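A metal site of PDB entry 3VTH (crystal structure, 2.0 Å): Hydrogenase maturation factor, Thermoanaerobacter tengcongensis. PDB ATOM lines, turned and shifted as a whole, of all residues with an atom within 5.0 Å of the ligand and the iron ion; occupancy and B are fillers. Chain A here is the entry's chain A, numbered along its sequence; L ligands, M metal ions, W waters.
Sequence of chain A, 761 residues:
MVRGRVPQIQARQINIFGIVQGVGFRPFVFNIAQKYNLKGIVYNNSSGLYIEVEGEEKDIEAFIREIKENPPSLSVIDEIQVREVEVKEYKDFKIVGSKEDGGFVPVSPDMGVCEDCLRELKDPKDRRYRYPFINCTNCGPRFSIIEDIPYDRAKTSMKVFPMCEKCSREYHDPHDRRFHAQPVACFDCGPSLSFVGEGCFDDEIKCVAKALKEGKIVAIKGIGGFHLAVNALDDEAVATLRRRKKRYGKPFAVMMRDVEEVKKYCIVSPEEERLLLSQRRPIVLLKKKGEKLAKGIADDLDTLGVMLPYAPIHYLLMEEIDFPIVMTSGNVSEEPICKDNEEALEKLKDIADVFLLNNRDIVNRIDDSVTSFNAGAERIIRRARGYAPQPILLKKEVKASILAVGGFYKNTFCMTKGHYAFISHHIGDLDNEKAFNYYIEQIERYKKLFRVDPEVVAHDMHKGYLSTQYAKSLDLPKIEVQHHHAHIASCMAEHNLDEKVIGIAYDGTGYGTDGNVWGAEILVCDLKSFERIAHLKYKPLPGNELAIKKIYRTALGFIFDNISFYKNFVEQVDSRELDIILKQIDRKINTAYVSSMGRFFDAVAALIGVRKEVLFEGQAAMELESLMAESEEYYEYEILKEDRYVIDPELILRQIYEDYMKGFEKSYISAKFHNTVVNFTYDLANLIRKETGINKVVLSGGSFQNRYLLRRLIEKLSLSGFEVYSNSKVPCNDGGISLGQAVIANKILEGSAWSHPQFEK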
ATOM      1  N   TYR A 409     -17.757  37.209 -28.765  1.00  0.00           N
ATOM      2  CA  TYR A 409     -16.599  37.219 -29.647  1.00  0.00           C
ATOM      3  C   TYR A 409     -17.004  36.908 -31.076  1.00  0.00           C
ATOM      4  O   TYR A 409     -17.860  36.052 -31.309  1.00  0.00           O
ATOM      5  CB  TYR A 409     -15.584  36.153 -29.236  1.00  0.00           C
ATOM      6  CG  TYR A 409     -14.914  36.406 -27.909  1.00  0.00           C
ATOM      7  CD1 TYR A 409     -13.945  37.397 -27.762  1.00  0.00           C
ATOM      8  CD2 TYR A 409     -15.249  35.630 -26.788  1.00  0.00           C
ATOM      9  CE1 TYR A 409     -13.306  37.620 -26.526  1.00  0.00           C
ATOM     10  CE2 TYR A 409     -14.623  35.851 -25.549  1.00  0.00           C
ATOM     11  CZ  TYR A 409     -13.661  36.839 -25.435  1.00  0.00           C
ATOM     12  OH  TYR A 409     -13.052  37.046 -24.215  1.00  0.00           O
ATOM     13  N   LYS A 410     -16.365  37.595 -32.024  1.00  0.00           N
ATOM     14  CA  LYS A 410     -16.492  37.238 -33.434  1.00  0.00           C
ATOM     15  C   LYS A 410     -17.964  37.132 -33.846  1.00  0.00           C
ATOM     16  O   LYS A 410     -18.376  36.213 -34.562  1.00  0.00           O
ATOM     17  CB  LYS A 410     -15.777  35.905 -33.701  1.00  0.00           C
ATOM     18  CG  LYS A 410     -14.240  35.938 -33.477  1.00  0.00           C
ATOM     19  CD  LYS A 410     -13.673  34.508 -33.565  1.00  0.00           C
ATOM     20  CE  LYS A 410     -12.132  34.434 -33.497  1.00  0.00           C
ATOM     21  NZ  LYS A 410     -11.534  35.054 -32.251  1.00  0.00           N
ATOM     22  N   TYR A 465     -23.923  39.275 -22.379  1.00  0.00           N
ATOM     23  CA  TYR A 465     -23.645  39.596 -23.797  1.00  0.00           C
ATOM     24  C   TYR A 465     -24.552  40.735 -24.228  1.00  0.00           C
ATOM     25  O   TYR A 465     -25.743  40.740 -23.934  1.00  0.00           O
ATOM     26  CB  TYR A 465     -23.919  38.397 -24.699  1.00  0.00           C
ATOM     27  CG  TYR A 465     -22.977  37.212 -24.567  1.00  0.00           C
ATOM     28  CD1 TYR A 465     -21.834  37.260 -23.736  1.00  0.00           C
ATOM     29  CD2 TYR A 465     -23.212  36.063 -25.293  1.00  0.00           C
ATOM     30  CE1 TYR A 465     -20.956  36.135 -23.651  1.00  0.00           C
ATOM     31  CE2 TYR A 465     -22.375  34.959 -25.208  1.00  0.00           C
ATOM     32  CZ  TYR A 465     -21.263  35.009 -24.382  1.00  0.00           C
ATOM     33  OH  TYR A 465     -20.485  33.869 -24.358  1.00  0.00           O
ATOM     34  N   HIS A 483     -24.478  27.763 -24.827  1.00  0.00           N
ATOM     35  CA  HIS A 483     -23.398  28.107 -25.773  1.00  0.00           C
ATOM     36  C   HIS A 483     -22.800  26.896 -26.499  1.00  0.00           C
ATOM     37  O   HIS A 483     -22.618  26.915 -27.720  1.00  0.00           O
ATOM     38  CB  HIS A 483     -22.281  28.828 -25.009  1.00  0.00           C
ATOM     39  CG  HIS A 483     -21.216  29.405 -25.878  1.00  0.00           C
ATOM     40  ND1 HIS A 483     -21.317  30.644 -26.470  1.00  0.00           N
ATOM     41  CD2 HIS A 483     -19.993  28.914 -26.229  1.00  0.00           C
ATOM     42  CE1 HIS A 483     -20.216  30.899 -27.161  1.00  0.00           C
ATOM     43  NE2 HIS A 483     -19.395  29.871 -27.028  1.00  0.00           N
ATOM     44  N   HIS A 487     -22.708  25.540 -30.467  1.00  0.00           N
ATOM     45  CA  HIS A 487     -21.523  25.145 -31.267  1.00  0.00           C
ATOM     46  C   HIS A 487     -21.782  23.799 -31.953  1.00  0.00           C
ATOM     47  O   HIS A 487     -21.549  23.647 -33.176  1.00  0.00           O
ATOM     48  CB  HIS A 487     -20.256  25.008 -30.386  1.00  0.00           C
ATOM     49  CG  HIS A 487     -19.490  26.279 -30.176  1.00  0.00           C
ATOM     50  ND1 HIS A 487     -19.052  27.079 -31.214  1.00  0.00           N
ATOM     51  CD2 HIS A 487     -19.020  26.854 -29.040  1.00  0.00           C
ATOM     52  CE1 HIS A 487     -18.354  28.093 -30.723  1.00  0.00           C
ATOM     53  NE2 HIS A 487     -18.336  27.978 -29.402  1.00  0.00           N
ATOM     54  N   ASP A 507     -13.714  25.063 -26.094  1.00  0.00           N
ATOM     55  CA  ASP A 507     -13.440  26.484 -26.357  1.00  0.00           C
ATOM     56  C   ASP A 507     -12.906  27.189 -25.102  1.00  0.00           C
ATOM     57  O   ASP A 507     -12.506  26.512 -24.163  1.00  0.00           O
ATOM     58  CB  ASP A 507     -14.643  27.223 -26.995  1.00  0.00           C
ATOM     59  CG  ASP A 507     -15.861  27.354 -26.081  1.00  0.00           C
ATOM     60  OD1 ASP A 507     -15.818  27.044 -24.861  1.00  0.00           O
ATOM     61  OD2 ASP A 507     -16.925  27.778 -26.603  1.00  0.00           O
ATOM     62  N   GLY A 508     -12.879  28.521 -25.125  1.00  0.00           N
ATOM     63  CA  GLY A 508     -12.379  29.305 -23.991  1.00  0.00           C
ATOM     64  C   GLY A 508     -13.386  29.546 -22.872  1.00  0.00           C
ATOM     65  O   GLY A 508     -13.148  29.198 -21.694  1.00  0.00           O
ATOM     66  N   THR A 509     -14.516  30.180 -23.204  1.00  0.00           N
ATOM     67  CA  THR A 509     -15.512  30.490 -22.185  1.00  0.00           C
ATOM     68  C   THR A 509     -16.893  30.507 -22.784  1.00  0.00           C
ATOM     69  O   THR A 509     -17.158  31.199 -23.759  1.00  0.00           O
ATOM     70  CB  THR A 509     -15.308  31.914 -21.555  1.00  0.00           C
ATOM     71  OG1 THR A 509     -15.202  32.881 -22.603  1.00  0.00           O
ATOM     72  CG2 THR A 509     -14.067  31.969 -20.709  1.00  0.00           C
ATOM     73  N   GLY A 510     -17.790  29.763 -22.174  1.00  0.00           N
ATOM     74  CA  GLY A 510     -19.195  29.837 -22.514  1.00  0.00           C
ATOM     75  C   GLY A 510     -19.898  29.675 -21.198  1.00  0.00           C
ATOM     76  O   GLY A 510     -19.396  29.001 -20.298  1.00  0.00           O
ATOM     77  N   GLY A 598      -9.655  26.178 -23.540  1.00  0.00           N
ATOM     78  CA  GLY A 598      -8.865  27.409 -23.740  1.00  0.00           C
ATOM     79  C   GLY A 598      -7.986  27.770 -22.546  1.00  0.00           C
ATOM     80  O   GLY A 598      -6.804  28.090 -22.704  1.00  0.00           O
ATOM     81  N   ARG A 599      -8.566  27.725 -21.346  1.00  0.00           N
ATOM     82  CA  ARG A 599      -7.813  28.026 -20.137  1.00  0.00           C
ATOM     83  C   ARG A 599      -6.772  26.942 -19.853  1.00  0.00           C
ATOM     84  O   ARG A 599      -5.687  27.237 -19.353  1.00  0.00           O
ATOM     85  CB  ARG A 599      -8.722  28.230 -18.910  1.00  0.00           C
ATOM     86  CG  ARG A 599      -9.770  29.381 -19.010  1.00  0.00           C
ATOM     87  CD  ARG A 599      -9.195  30.815 -19.135  1.00  0.00           C
ATOM     88  NE  ARG A 599      -8.547  31.014 -20.438  1.00  0.00           N
ATOM     89  CZ  ARG A 599      -9.178  31.372 -21.560  1.00  0.00           C
ATOM     90  NH1 ARG A 599     -10.482  31.612 -21.560  1.00  0.00           N
ATOM     91  NH2 ARG A 599      -8.490  31.492 -22.683  1.00  0.00           N
ATOM     92  N   PHE A 601      -5.140  25.244 -22.149  1.00  0.00           N
ATOM     93  CA  PHE A 601      -4.035  25.670 -23.015  1.00  0.00           C
ATOM     94  C   PHE A 601      -3.245  26.837 -22.424  1.00  0.00           C
ATOM     95  O   PHE A 601      -2.018  26.800 -22.419  1.00  0.00           O
ATOM     96  CB  PHE A 601      -4.536  26.033 -24.437  1.00  0.00           C
ATOM     97  CG  PHE A 601      -4.485  24.878 -25.394  1.00  0.00           C
ATOM     98  CD1 PHE A 601      -3.573  24.886 -26.450  1.00  0.00           C
ATOM     99  CD2 PHE A 601      -5.349  23.791 -25.248  1.00  0.00           C
ATOM    100  CE1 PHE A 601      -3.528  23.815 -27.374  1.00  0.00           C
ATOM    101  CE2 PHE A 601      -5.310  22.715 -26.164  1.00  0.00           C
ATOM    102  CZ  PHE A 601      -4.389  22.722 -27.217  1.00  0.00           C
ATOM    103  N   GLU A 617      -6.920  37.401 -26.851  1.00  0.00           N
ATOM    104  CA  GLU A 617      -7.470  36.126 -26.400  1.00  0.00           C
ATOM    105  C   GLU A 617      -7.046  35.005 -27.372  1.00  0.00           C
ATOM    106  O   GLU A 617      -7.250  35.115 -28.577  1.00  0.00           O
ATOM    107  CB  GLU A 617      -9.002  36.255 -26.322  1.00  0.00           C
ATOM    108  CG  GLU A 617      -9.780  35.020 -25.875  1.00  0.00           C
ATOM    109  CD  GLU A 617      -9.922  34.899 -24.354  1.00  0.00           C
ATOM    110  OE1 GLU A 617      -8.907  34.582 -23.679  1.00  0.00           O
ATOM    111  OE2 GLU A 617     -11.050  35.091 -23.840  1.00  0.00           O
ATOM    112  N   GLY A 618      -6.445  33.946 -26.840  1.00  0.00           N
ATOM    113  CA  GLY A 618      -6.075  32.810 -27.669  1.00  0.00           C
ATOM    114  C   GLY A 618      -4.644  32.850 -28.167  1.00  0.00           C
ATOM    115  O   GLY A 618      -4.143  31.861 -28.702  1.00  0.00           O
ATOM    116  N   ALA A 621      -2.498  30.079 -26.890  1.00  0.00           N
ATOM    117  CA  ALA A 621      -2.831  28.757 -27.463  1.00  0.00           C
ATOM    118  C   ALA A 621      -2.291  28.597 -28.891  1.00  0.00           C
ATOM    119  O   ALA A 621      -1.817  27.511 -29.261  1.00  0.00           O
ATOM    120  CB  ALA A 621      -4.331  28.480 -27.380  1.00  0.00           C
ATOM    121  N   MET A 622      -2.326  29.671 -29.673  1.00  0.00           N
ATOM    122  CA  MET A 622      -1.760  29.693 -31.016  1.00  0.00           C
ATOM    123  C   MET A 622      -0.246  29.480 -31.008  1.00  0.00           C
ATOM    124  O   MET A 622       0.280  28.748 -31.828  1.00  0.00           O
ATOM    125  CB  MET A 622      -2.119  31.009 -31.717  1.00  0.00           C
ATOM    126  CG  MET A 622      -3.628  31.149 -31.978  1.00  0.00           C
ATOM    127  SD  MET A 622      -4.099  32.805 -32.535  1.00  0.00           S
ATOM    128  CE  MET A 622      -3.412  32.771 -34.193  1.00  0.00           C
ATOM    129  N   GLU A 625       0.592  25.798 -30.120  1.00  0.00           N
ATOM    130  CA  GLU A 625       0.399  24.950 -31.305  1.00  0.00           C
ATOM    131  C   GLU A 625       1.520  25.121 -32.329  1.00  0.00           C
ATOM    132  O   GLU A 625       2.017  24.130 -32.881  1.00  0.00           O
ATOM    133  CB  GLU A 625      -0.965  25.224 -31.968  1.00  0.00           C
ATOM    134  CG  GLU A 625      -1.265  24.269 -33.154  1.00  0.00           C
ATOM    135  CD  GLU A 625      -2.400  24.730 -34.087  1.00  0.00           C
ATOM    136  OE1 GLU A 625      -3.005  25.787 -33.835  1.00  0.00           O
ATOM    137  OE2 GLU A 625      -2.670  24.028 -35.089  1.00  0.00           O
ATOM    138  N   GLY A 701     -16.527  24.421 -31.388  1.00  0.00           N
ATOM    139  CA  GLY A 701     -15.949  25.286 -30.368  1.00  0.00           C
ATOM    140  C   GLY A 701     -14.609  25.759 -30.879  1.00  0.00           C
ATOM    141  O   GLY A 701     -13.956  25.066 -31.658  1.00  0.00           O
ATOM    142  N   GLY A 702     -14.192  26.926 -30.412  1.00  0.00           N
ATOM    143  CA  GLY A 702     -13.002  27.605 -30.910  1.00  0.00           C
ATOM    144  C   GLY A 702     -11.671  26.868 -30.709  1.00  0.00           C
ATOM    145  O   GLY A 702     -10.729  27.141 -31.441  1.00  0.00           O
ATOM    146  N   SER A 703     -11.584  25.938 -29.753  1.00  0.00           N
ATOM    147  CA  SER A 703     -10.342  25.150 -29.628  1.00  0.00           C
ATOM    148  C   SER A 703     -10.082  24.306 -30.890  1.00  0.00           C
ATOM    149  O   SER A 703      -8.953  23.944 -31.171  1.00  0.00           O
ATOM    150  CB  SER A 703     -10.369  24.220 -28.399  1.00  0.00           C
ATOM    151  OG  SER A 703     -10.528  24.922 -27.184  1.00  0.00           O
ATOM    152  N   GLN A 705     -10.129  25.320 -33.870  1.00  0.00           N
ATOM    153  CA  GLN A 705      -9.243  26.079 -34.747  1.00  0.00           C
ATOM    154  C   GLN A 705      -7.809  25.540 -34.721  1.00  0.00           C
ATOM    155  O   GLN A 705      -7.018  25.817 -35.629  1.00  0.00           O
ATOM    156  CB  GLN A 705      -9.244  27.549 -34.371  1.00  0.00           C
ATOM    157  CG  GLN A 705     -10.589  28.249 -34.630  1.00  0.00           C
ATOM    158  CD  GLN A 705     -10.632  29.614 -33.997  1.00  0.00           C
ATOM    159  OE1 GLN A 705     -10.592  29.743 -32.756  1.00  0.00           O
ATOM    160  NE2 GLN A 705     -10.713  30.643 -34.823  1.00  0.00           N
ATOM    161  N   ASN A 706      -7.476  24.783 -33.687  1.00  0.00           N
ATOM    162  CA  ASN A 706      -6.174  24.103 -33.605  1.00  0.00           C
ATOM    163  C   ASN A 706      -6.172  22.976 -34.656  1.00  0.00           C
ATOM    164  O   ASN A 706      -6.966  22.024 -34.559  1.00  0.00           O
ATOM    165  CB  ASN A 706      -6.008  23.535 -32.192  1.00  0.00           C
ATOM    166  CG  ASN A 706      -4.640  22.947 -31.944  1.00  0.00           C
ATOM    167  OD1 ASN A 706      -4.192  22.051 -32.645  1.00  0.00           O
ATOM    168  ND2 ASN A 706      -3.948  23.474 -30.932  1.00  0.00           N
ATOM    169  N   LEU A 709      -5.258  19.269 -33.158  1.00  0.00           N
ATOM    170  CA  LEU A 709      -6.396  18.702 -32.411  1.00  0.00           C
ATOM    171  C   LEU A 709      -7.506  18.208 -33.328  1.00  0.00           C
ATOM    172  O   LEU A 709      -8.003  17.095 -33.173  1.00  0.00           O
ATOM    173  CB  LEU A 709      -7.008  19.722 -31.435  1.00  0.00           C
ATOM    174  CG  LEU A 709      -6.272  20.152 -30.172  1.00  0.00           C
ATOM    175  CD1 LEU A 709      -7.209  20.962 -29.294  1.00  0.00           C
ATOM    176  CD2 LEU A 709      -5.694  18.959 -29.387  1.00  0.00           C
ATOM    177  N   CYS A 732     -15.960  27.037 -36.402  1.00  0.00           N
ATOM    178  CA  CYS A 732     -16.137  26.322 -35.155  1.00  0.00           C
ATOM    179  C   CYS A 732     -15.971  27.296 -33.991  1.00  0.00           C
ATOM    180  O   CYS A 732     -16.340  26.990 -32.864  1.00  0.00           O
ATOM    181  CB  CYS A 732     -15.154  25.135 -35.038  1.00  0.00           C
ATOM    182  SG  CYS A 732     -13.400  25.629 -35.037  1.00  0.00           S
ATOM    183  N   ASN A 733     -15.418  28.482 -34.267  1.00  0.00           N
ATOM    184  CA  ASN A 733     -15.360  29.550 -33.252  1.00  0.00           C
ATOM    185  C   ASN A 733     -16.715  30.246 -33.105  1.00  0.00           C
ATOM    186  O   ASN A 733     -17.680  29.838 -33.741  1.00  0.00           O
ATOM    187  CB  ASN A 733     -14.220  30.533 -33.519  1.00  0.00           C
ATOM    188  CG  ASN A 733     -14.413  31.338 -34.807  1.00  0.00           C
ATOM    189  OD1 ASN A 733     -15.492  31.882 -35.079  1.00  0.00           O
ATOM    190  ND2 ASN A 733     -13.345  31.425 -35.608  1.00  0.00           N
ATOM    191  N   ASP A 734     -16.786  31.272 -32.266  1.00  0.00           N
ATOM    192  CA  ASP A 734     -18.087  31.894 -31.967  1.00  0.00           C
ATOM    193  C   ASP A 734     -18.797  32.558 -33.143  1.00  0.00           C
ATOM    194  O   ASP A 734     -19.982  32.891 -33.037  1.00  0.00           O
ATOM    195  CB  ASP A 734     -17.962  32.871 -30.789  1.00  0.00           C
ATOM    196  CG  ASP A 734     -17.912  32.155 -29.446  1.00  0.00           C
ATOM    197  OD1 ASP A 734     -17.898  30.905 -29.441  1.00  0.00           O
ATOM    198  OD2 ASP A 734     -17.890  32.832 -28.396  1.00  0.00           O
ATOM    199  N   ILE A 737     -21.827  30.409 -33.879  1.00  0.00           N
ATOM    200  CA  ILE A 737     -22.842  30.214 -32.827  1.00  0.00           C
ATOM    201  C   ILE A 737     -24.286  30.530 -33.288  1.00  0.00           C
ATOM    202  O   ILE A 737     -25.196  29.792 -32.990  1.00  0.00           O
ATOM    203  CB  ILE A 737     -22.470  31.042 -31.576  1.00  0.00           C
ATOM    204  CG1 ILE A 737     -21.316  30.364 -30.787  1.00  0.00           C
ATOM    205  CG2 ILE A 737     -23.660  31.355 -30.695  1.00  0.00           C
ATOM    206  CD1 ILE A 737     -21.705  29.085 -30.018  1.00  0.00           C
HETATM  207  P1  LIG L   1     -15.566  31.465 -26.357  1.00  0.00           P
HETATM  208  O1  LIG L   1     -14.343  30.801 -25.769  1.00  0.00           O
HETATM  209  O2  LIG L   1     -16.753  30.592 -26.603  1.00  0.00           O
HETATM  210  O3  LIG L   1     -15.880  32.776 -25.667  1.00  0.00           O
HETATM  211  C1  LIG L   1     -14.980  31.972 -27.998  1.00  0.00           C
HETATM  212  P2  LIG L   1     -14.621  30.613 -29.143  1.00  0.00           P
HETATM  213  O4  LIG L   1     -14.420  31.379 -30.437  1.00  0.00           O
HETATM  214  O5  LIG L   1     -15.578  29.447 -29.106  1.00  0.00           O
HETATM  215  O6  LIG L   1     -13.207  30.021 -28.626  1.00  0.00           O
HETATM  216  C2  LIG L   1     -12.049  30.828 -28.787  1.00  0.00           C
HETATM  217  C3  LIG L   1     -11.000  30.196 -27.905  1.00  0.00           C
HETATM  218  O7  LIG L   1     -10.522  28.989 -28.505  1.00  0.00           O
HETATM  219  C4  LIG L   1      -9.767  31.066 -27.751  1.00  0.00           C
HETATM  220  O8  LIG L   1      -9.989  32.108 -26.788  1.00  0.00           O
HETATM  221  C5  LIG L   1      -8.753  30.035 -27.320  1.00  0.00           C
HETATM  222  O9  LIG L   1      -8.937  29.839 -25.912  1.00  0.00           O
HETATM  223  C6  LIG L   1      -9.168  28.777 -28.109  1.00  0.00           C
HETATM  224  N1  LIG L   1      -8.227  28.658 -29.263  1.00  0.00           N
HETATM  225  C7  LIG L   1      -8.094  29.510 -30.309  1.00  0.00           C
HETATM  226  N2  LIG L   1      -7.108  29.117 -31.145  1.00  0.00           N
HETATM  227  C8  LIG L   1      -6.590  27.973 -30.651  1.00  0.00           C
HETATM  228  C9  LIG L   1      -5.520  27.026 -31.042  1.00  0.00           C
HETATM  229  N3  LIG L   1      -4.783  27.205 -32.165  1.00  0.00           N
HETATM  230  N4  LIG L   1      -5.294  25.969 -30.219  1.00  0.00           N
HETATM  231  C10 LIG L   1      -6.017  25.747 -29.099  1.00  0.00           C
HETATM  232  N5  LIG L   1      -7.003  26.578 -28.683  1.00  0.00           N
HETATM  233  C11 LIG L   1      -7.324  27.687 -29.403  1.00  0.00           C
HETATM  234 FE    FE M   1     -17.459  29.333 -27.931  1.00  0.00          FE
HETATM  235  O   HOH W   1      -6.852  30.994 -33.060  1.00  0.00           O
HETATM  236  O   HOH W   2      -8.063  25.667 -26.553  1.00  0.00           O
HETATM  237  O   HOH W   3      -6.408  29.938 -24.798  1.00  0.00           O
HETATM  238  O   HOH W   4     -12.208  32.744 -24.633  1.00  0.00           O
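Tyr 409 touches the ligand.
Gly 598 touches the ligand.
Arg 599 touches the ligand.
Phe 601 touches the ligand (CE1 to C10, 3.6 Å).
CG of Glu 617 touches O8 of the ligand, 3.1 Å away.
CA of Gly 618 touches C5 of the ligand, at 3.9 Å.
Ala 621 touches the ligand (CB to N5, 3.5 Å).
Gln 705 touches the ligand (OE1 to C7, 3.5 Å).
Asn 733 touches the ligand.
Hydrophobic or aromatic side chains that line the ligand: Tyr 409, His 483, His 487, Phe 601 and Ala 621.
Within 4 Å of the ligand: Tyr 409, His 483, His 487, Asp 507, Gly 508, Thr 509, Gly 598, Arg 599, Phe 601, Glu 617, Gly 618, Ala 621, Glu 625, Gly 702, Ser 703, Gln 705, Asn 706, Asn 733 and Asp 734.
A ring nitrogen (ND1) of His 487 lies close to the backbone carbonyl oxygen (O) of Cys 732, at 3.2 Å.
OE2 of Glu 625 sits close to OD1 of Asn 706 (3.5 Å).
OD1 of Asn 706 is in hydrogen-bond range of N of Leu 709 (3.0 Å).
OE2 of Glu 617 lies within hydrogen-bond range of OH of Tyr 409 (2.8 Å).
The side-chain carboxylate of Glu 617 lies within salt-bridge range of the guanidinium group of Arg 599.
The side-chain amide oxygen of Gln 705 sits close to the backbone carbonyl oxygen of Gly 702, 2.9 Å away.
The backbone carbonyl oxygen (O) of Cys 732 is in hydrogen-bond range of the backbone NH (N) of Gly 702, 3.3 Å away.
The side-chain amide nitrogen (NE2) of Gln 705 lies close to the side-chain amide nitrogen (ND2) of Asn 733, at 2.9 Å.
The backbone NH (N) of Asp 734 sits at hydrogen-bond distance from an oxygen (O4) of the ligand (3.0 Å).
The backbone NH of Thr 509 lies within hydrogen-bond range of an oxygen (O1) of the ligand, 2.6 Å away.
The backbone carbonyl oxygen (O) of Thr 509 sits close to an oxygen (O3) of the ligand (2.8 Å).
OG1 of Thr 509 sits at hydrogen-bond distance from O3 of the ligand (3.1 Å).
N of Gly 508 is in hydrogen-bond range of O1 of the ligand, 2.8 Å away.
OE1 of Glu 625 sits at hydrogen-bond distance from N3 of the ligand.
A nitrogen (N4) of the ligand lies within hydrogen-bond range of the side-chain amide nitrogen (ND2) of Asn 706.
The backbone NH (N) of Gly 702 sits close to an oxygen (O5) of the ligand (3.2 Å).
O7 of the ligand is in hydrogen-bond range of N of Ser 703 (3.5 Å).
The iron ion is bound by an oxygen (O2) of the ligand, at 2.0 Å.
OD2 of Asp 507 is bound to the iron ion, 2.1 Å away.
NE2 of His 487 is bound to the iron ion (2.2 Å).
The iron ion is bound by a ring nitrogen (NE2) of His 483 (2.2 Å).
O5 of the ligand binds the iron ion.
OD1 of Asp 734 is bound to the iron ion.
The iron ion has six donor atoms within binding distance.
Water W2 lies within hydrogen-bond range of a nitrogen (N5) of the ligand (2.5 Å), the side-chain hydroxyl (OG) of Ser 703 (2.7 Å) and the backbone NH (N) of Gly 598 (3.4 Å).
Water W1 bridges a nitrogen (N2) of the ligand and the side-chain sulfur (SD) of Met 622.
Water W3 lies within hydrogen-bond range of an oxygen (O9) of the ligand (2.8 Å), the backbone carbonyl oxygen of Gly 598 (2.8 Å) and the guanidinium group of Arg 599 (3.4 Å).
Water W4 bridges the side-chain carboxylate (OE2) of Glu 617 (2.7 Å) and an oxygen (O1) of the ligand (3.1 Å).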
